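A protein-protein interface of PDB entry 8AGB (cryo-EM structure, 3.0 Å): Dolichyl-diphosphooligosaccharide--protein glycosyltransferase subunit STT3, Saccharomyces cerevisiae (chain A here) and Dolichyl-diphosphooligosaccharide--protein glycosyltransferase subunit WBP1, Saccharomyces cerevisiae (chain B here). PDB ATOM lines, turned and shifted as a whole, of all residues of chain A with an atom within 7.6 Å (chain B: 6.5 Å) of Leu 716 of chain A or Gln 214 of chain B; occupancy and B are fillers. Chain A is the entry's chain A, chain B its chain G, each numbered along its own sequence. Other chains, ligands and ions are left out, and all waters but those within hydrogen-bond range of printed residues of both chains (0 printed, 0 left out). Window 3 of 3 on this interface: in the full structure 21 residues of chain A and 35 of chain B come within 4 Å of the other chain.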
ATOM      1  N   ARG A 711     -10.790 -20.528 -10.133  1.00  0.00           N
ATOM      2  CA  ARG A 711     -10.446 -20.546 -11.546  1.00  0.00           C
ATOM      3  C   ARG A 711      -8.958 -20.242 -11.727  1.00  0.00           C
ATOM      4  O   ARG A 711      -8.475 -19.220 -11.221  1.00  0.00           O
ATOM      5  CB  ARG A 711     -11.288 -19.520 -12.304  1.00  0.00           C
ATOM      6  CG  ARG A 711     -11.544 -19.861 -13.757  1.00  0.00           C
ATOM      7  CD  ARG A 711     -12.586 -18.931 -14.347  1.00  0.00           C
ATOM      8  NE  ARG A 711     -12.975 -19.324 -15.695  1.00  0.00           N
ATOM      9  CZ  ARG A 711     -12.291 -19.001 -16.788  1.00  0.00           C
ATOM     10  NH1 ARG A 711     -11.185 -18.278 -16.694  1.00  0.00           N
ATOM     11  NH2 ARG A 711     -12.718 -19.402 -17.977  1.00  0.00           N
ATOM     12  N   LEU A 714      -6.012 -19.215 -16.697  1.00  0.00           N
ATOM     13  CA  LEU A 714      -5.090 -19.606 -17.754  1.00  0.00           C
ATOM     14  C   LEU A 714      -5.361 -18.765 -18.999  1.00  0.00           C
ATOM     15  O   LEU A 714      -6.166 -17.829 -18.986  1.00  0.00           O
ATOM     16  CB  LEU A 714      -5.226 -21.097 -18.044  1.00  0.00           C
ATOM     17  CG  LEU A 714      -5.219 -22.038 -16.841  1.00  0.00           C
ATOM     18  CD1 LEU A 714      -5.823 -23.371 -17.220  1.00  0.00           C
ATOM     19  CD2 LEU A 714      -3.807 -22.224 -16.318  1.00  0.00           C
ATOM     20  N   GLY A 715      -4.685 -19.090 -20.102  1.00  0.00           N
ATOM     21  CA  GLY A 715      -4.922 -18.451 -21.374  1.00  0.00           C
ATOM     22  C   GLY A 715      -5.679 -19.369 -22.321  1.00  0.00           C
ATOM     23  O   GLY A 715      -5.992 -20.515 -22.010  1.00  0.00           O
ATOM     24  N   LEU A 716      -5.975 -18.829 -23.501  1.00  0.00           N
ATOM     25  CA  LEU A 716      -6.789 -19.567 -24.456  1.00  0.00           C
ATOM     26  C   LEU A 716      -6.069 -20.822 -24.930  1.00  0.00           C
ATOM     27  O   LEU A 716      -4.900 -20.771 -25.323  1.00  0.00           O
ATOM     28  CB  LEU A 716      -7.116 -18.677 -25.653  1.00  0.00           C
ATOM     29  CG  LEU A 716      -8.523 -18.099 -25.769  1.00  0.00           C
ATOM     30  CD1 LEU A 716      -9.059 -17.706 -24.405  1.00  0.00           C
ATOM     31  CD2 LEU A 716      -8.497 -16.903 -26.703  1.00  0.00           C
ATOM     32  N   ARG A 717      -6.769 -21.951 -24.886  1.00  0.00           N
ATOM     33  CA  ARG A 717      -6.232 -23.186 -25.440  1.00  0.00           C
ATOM     34  C   ARG A 717      -6.185 -23.064 -26.956  1.00  0.00           C
ATOM     35  O   ARG A 717      -7.221 -22.838 -27.590  1.00  0.00           O
ATOM     36  CB  ARG A 717      -7.082 -24.378 -25.012  1.00  0.00           C
ATOM     37  CG  ARG A 717      -6.825 -25.635 -25.813  1.00  0.00           C
ATOM     38  CD  ARG A 717      -5.754 -26.474 -25.149  1.00  0.00           C
ATOM     39  NE  ARG A 717      -5.163 -27.443 -26.063  1.00  0.00           N
ATOM     40  CZ  ARG A 717      -4.181 -28.272 -25.731  1.00  0.00           C
ATOM     41  NH1 ARG A 717      -3.685 -28.252 -24.504  1.00  0.00           N
ATOM     42  NH2 ARG A 717      -3.698 -29.125 -26.621  1.00  0.00           N
ATOM     43  N   VAL A 718      -4.993 -23.172 -27.533  1.00  0.00           N
ATOM     44  CA  VAL A 718      -4.816 -23.134 -28.986  1.00  0.00           C
ATOM     45  C   VAL A 718      -5.872 -23.940 -29.739  1.00  0.00           C
ATOM     46  O   VAL A 718      -5.750 -24.170 -30.942  1.00  0.00           O
ATOM     47  CB  VAL A 718      -3.416 -23.602 -29.373  1.00  0.00           C
ATOM     48  CG1 VAL A 718      -2.389 -22.771 -28.642  1.00  0.00           C
ATOM     49  CG2 VAL A 718      -3.243 -25.076 -29.054  1.00  0.00           C
ATOM     50  N   ALA B 180     -14.416 -28.511 -18.579  1.00  0.00           N
ATOM     51  CA  ALA B 180     -13.099 -28.480 -17.963  1.00  0.00           C
ATOM     52  C   ALA B 180     -12.206 -27.527 -18.737  1.00  0.00           C
ATOM     53  O   ALA B 180     -12.267 -27.472 -19.966  1.00  0.00           O
ATOM     54  CB  ALA B 180     -12.460 -29.867 -17.923  1.00  0.00           C
ATOM     55  N   LEU B 181     -11.379 -26.783 -18.014  1.00  0.00           N
ATOM     56  CA  LEU B 181     -10.371 -25.952 -18.649  1.00  0.00           C
ATOM     57  C   LEU B 181      -9.106 -26.768 -18.880  1.00  0.00           C
ATOM     58  O   LEU B 181      -8.891 -27.815 -18.264  1.00  0.00           O
ATOM     59  CB  LEU B 181     -10.057 -24.724 -17.797  1.00  0.00           C
ATOM     60  CG  LEU B 181     -11.235 -23.828 -17.423  1.00  0.00           C
ATOM     61  CD1 LEU B 181     -10.761 -22.676 -16.559  1.00  0.00           C
ATOM     62  CD2 LEU B 181     -11.928 -23.313 -18.672  1.00  0.00           C
ATOM     63  N   LEU B 182      -8.235 -26.245 -19.738  1.00  0.00           N
ATOM     64  CA  LEU B 182      -7.063 -26.985 -20.179  1.00  0.00           C
ATOM     65  C   LEU B 182      -5.864 -26.061 -20.312  1.00  0.00           C
ATOM     66  O   LEU B 182      -5.987 -24.932 -20.792  1.00  0.00           O
ATOM     67  CB  LEU B 182      -7.321 -27.660 -21.535  1.00  0.00           C
ATOM     68  CG  LEU B 182      -7.731 -29.129 -21.659  1.00  0.00           C
ATOM     69  CD1 LEU B 182      -9.018 -29.429 -20.932  1.00  0.00           C
ATOM     70  CD2 LEU B 182      -7.882 -29.477 -23.124  1.00  0.00           C
ATOM     71  N   ASN B 184      -1.883 -25.559 -21.959  1.00  0.00           N
ATOM     72  CA  ASN B 184      -1.297 -25.789 -23.276  1.00  0.00           C
ATOM     73  C   ASN B 184      -0.107 -26.738 -23.153  1.00  0.00           C
ATOM     74  O   ASN B 184       1.059 -26.354 -23.238  1.00  0.00           O
ATOM     75  CB  ASN B 184      -0.900 -24.466 -23.917  1.00  0.00           C
ATOM     76  CG  ASN B 184      -2.000 -23.893 -24.774  1.00  0.00           C
ATOM     77  OD1 ASN B 184      -2.105 -24.211 -25.953  1.00  0.00           O
ATOM     78  ND2 ASN B 184      -2.828 -23.039 -24.187  1.00  0.00           N
ATOM     79  N   ASN B 193     -15.813 -30.922 -27.351  1.00  0.00           N
ATOM     80  CA  ASN B 193     -15.800 -29.490 -27.100  1.00  0.00           C
ATOM     81  C   ASN B 193     -17.218 -29.056 -26.774  1.00  0.00           C
ATOM     82  O   ASN B 193     -18.189 -29.714 -27.154  1.00  0.00           O
ATOM     83  CB  ASN B 193     -15.263 -28.724 -28.312  1.00  0.00           C
ATOM     84  CG  ASN B 193     -14.360 -27.581 -27.924  1.00  0.00           C
ATOM     85  OD1 ASN B 193     -14.130 -27.330 -26.744  1.00  0.00           O
ATOM     86  ND2 ASN B 193     -13.837 -26.880 -28.921  1.00  0.00           N
ATOM     87  N   ALA B 194     -17.329 -27.952 -26.071  1.00  0.00           N
ATOM     88  CA  ALA B 194     -18.674 -27.535 -25.723  1.00  0.00           C
ATOM     89  C   ALA B 194     -19.252 -26.672 -26.832  1.00  0.00           C
ATOM     90  O   ALA B 194     -18.510 -26.086 -27.625  1.00  0.00           O
ATOM     91  CB  ALA B 194     -18.661 -26.766 -24.406  1.00  0.00           C
ATOM     92  N   THR B 210     -16.384 -22.009 -17.391  1.00  0.00           N
ATOM     93  CA  THR B 210     -16.091 -22.035 -18.815  1.00  0.00           C
ATOM     94  C   THR B 210     -17.144 -21.231 -19.562  1.00  0.00           C
ATOM     95  O   THR B 210     -18.242 -20.983 -19.057  1.00  0.00           O
ATOM     96  CB  THR B 210     -16.038 -23.466 -19.359  1.00  0.00           C
ATOM     97  OG1 THR B 210     -17.351 -23.880 -19.752  1.00  0.00           O
ATOM     98  CG2 THR B 210     -15.501 -24.408 -18.306  1.00  0.00           C
ATOM     99  N   SER B 211     -16.797 -20.824 -20.780  1.00  0.00           N
ATOM    100  CA  SER B 211     -17.714 -20.064 -21.624  1.00  0.00           C
ATOM    101  C   SER B 211     -17.369 -20.350 -23.077  1.00  0.00           C
ATOM    102  O   SER B 211     -16.323 -19.906 -23.560  1.00  0.00           O
ATOM    103  CB  SER B 211     -17.629 -18.572 -21.323  1.00  0.00           C
ATOM    104  OG  SER B 211     -18.356 -17.820 -22.279  1.00  0.00           O
ATOM    105  N   GLY B 212     -18.234 -21.087 -23.767  1.00  0.00           N
ATOM    106  CA  GLY B 212     -18.047 -21.278 -25.190  1.00  0.00           C
ATOM    107  C   GLY B 212     -17.133 -22.438 -25.513  1.00  0.00           C
ATOM    108  O   GLY B 212     -17.035 -23.394 -24.740  1.00  0.00           O
ATOM    109  N   SER B 213     -16.452 -22.363 -26.654  1.00  0.00           N
ATOM    110  CA  SER B 213     -15.657 -23.472 -27.160  1.00  0.00           C
ATOM    111  C   SER B 213     -14.299 -23.582 -26.487  1.00  0.00           C
ATOM    112  O   SER B 213     -13.440 -24.325 -26.974  1.00  0.00           O
ATOM    113  CB  SER B 213     -15.474 -23.346 -28.673  1.00  0.00           C
ATOM    114  OG  SER B 213     -16.598 -23.867 -29.360  1.00  0.00           O
ATOM    115  N   GLN B 214     -14.081 -22.857 -25.393  1.00  0.00           N
ATOM    116  CA  GLN B 214     -12.885 -23.009 -24.580  1.00  0.00           C
ATOM    117  C   GLN B 214     -13.127 -23.900 -23.372  1.00  0.00           C
ATOM    118  O   GLN B 214     -12.255 -24.009 -22.506  1.00  0.00           O
ATOM    119  CB  GLN B 214     -12.366 -21.643 -24.134  1.00  0.00           C
ATOM    120  CG  GLN B 214     -11.627 -20.900 -25.220  1.00  0.00           C
ATOM    121  CD  GLN B 214     -10.255 -21.484 -25.465  1.00  0.00           C
ATOM    122  OE1 GLN B 214      -9.784 -21.543 -26.599  1.00  0.00           O
ATOM    123  NE2 GLN B 214      -9.607 -21.928 -24.398  1.00  0.00           N
ATOM    124  N   GLY B 215     -14.292 -24.533 -23.300  1.00  0.00           N
ATOM    125  CA  GLY B 215     -14.593 -25.496 -22.263  1.00  0.00           C
ATOM    126  C   GLY B 215     -14.795 -26.851 -22.900  1.00  0.00           C
ATOM    127  O   GLY B 215     -15.577 -26.977 -23.844  1.00  0.00           O
ATOM    128  N   PHE B 216     -14.098 -27.869 -22.412  1.00  0.00           N
ATOM    129  CA  PHE B 216     -14.097 -29.174 -23.052  1.00  0.00           C
ATOM    130  C   PHE B 216     -15.014 -30.135 -22.312  1.00  0.00           C
ATOM    131  O   PHE B 216     -15.200 -30.036 -21.098  1.00  0.00           O
ATOM    132  CB  PHE B 216     -12.677 -29.730 -23.124  1.00  0.00           C
ATOM    133  CG  PHE B 216     -11.778 -28.940 -24.024  1.00  0.00           C
ATOM    134  CD1 PHE B 216     -11.120 -27.819 -23.556  1.00  0.00           C
ATOM    135  CD2 PHE B 216     -11.616 -29.297 -25.347  1.00  0.00           C
ATOM    136  CE1 PHE B 216     -10.303 -27.083 -24.386  1.00  0.00           C
ATOM    137  CE2 PHE B 216     -10.802 -28.563 -26.180  1.00  0.00           C
ATOM    138  CZ  PHE B 216     -10.144 -27.455 -25.698  1.00  0.00           C
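N of Val 718 of chain A lies close to OD1 of Asn 184 of chain B (3.5 Å). The side-chain amide nitrogen (ND2) of Asn 184 of chain B is in hydrogen-bond range of the backbone carbonyl oxygen (O) of Leu 716 of chain A (3.3 Å). N of Arg 717 of chain A lies close to NE2 of Gln 214 of chain B (2.9 Å).
O of Phe 216 of chain B sits at hydrogen-bond distance from N of Ala 180 of chain B, at 3.0 Å.
Arg 711 of chain A touches Leu 181 of chain B (CZ to CD1, 3.99 Å). CD1 of Leu 714 of chain A touches O of Leu 182 of chain B, at 3.9 Å. CA of Leu 716 of chain A touches NE2 of Gln 214 of chain B, 3.7 Å away. Asn 184 of chain B touches Arg 717 of chain A (ND2 to CA, 3.6 Å). Arg 717 of chain A touches Phe 216 of chain B.
Of chain B, only Asn 184 and Gln 214 come within 4 Å of Leu 716 of chain A. Of chain A, only Leu 716 (3.7 Å) and Arg 717 (2.9 Å) come within 4 Å of Gln 214 of chain B. Printed residues of chain A within 4 Å of Asn 184 of chain B: Leu 716 (3.3 Å), Arg 717 (3.6 Å) and Val 718 (3.1 Å). Of the printed residues of chain B, Arg 711 of chain A touches Leu 181. Printed residues of chain A within 4 Å of Leu 182 of chain B: Leu 714 (3.9 Å). Of the printed residues of chain B, Arg 717 of chain A touches Asn 184, Gln 214 and Phe 216. Printed residues of chain A within 4 Å of Leu 181 of chain B: Arg 711. Ala 194 of chain B touches none of the printed residues of chain A. Gly 715 of chain A touches none of the printed residues of chain B.
Among the printed residues, 8 pairs touch across the chains. Among the printed residues, no Asp or Glu carboxylate lies within 4 Å of a Lys or Arg side-chain nitrogen of the other chain.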
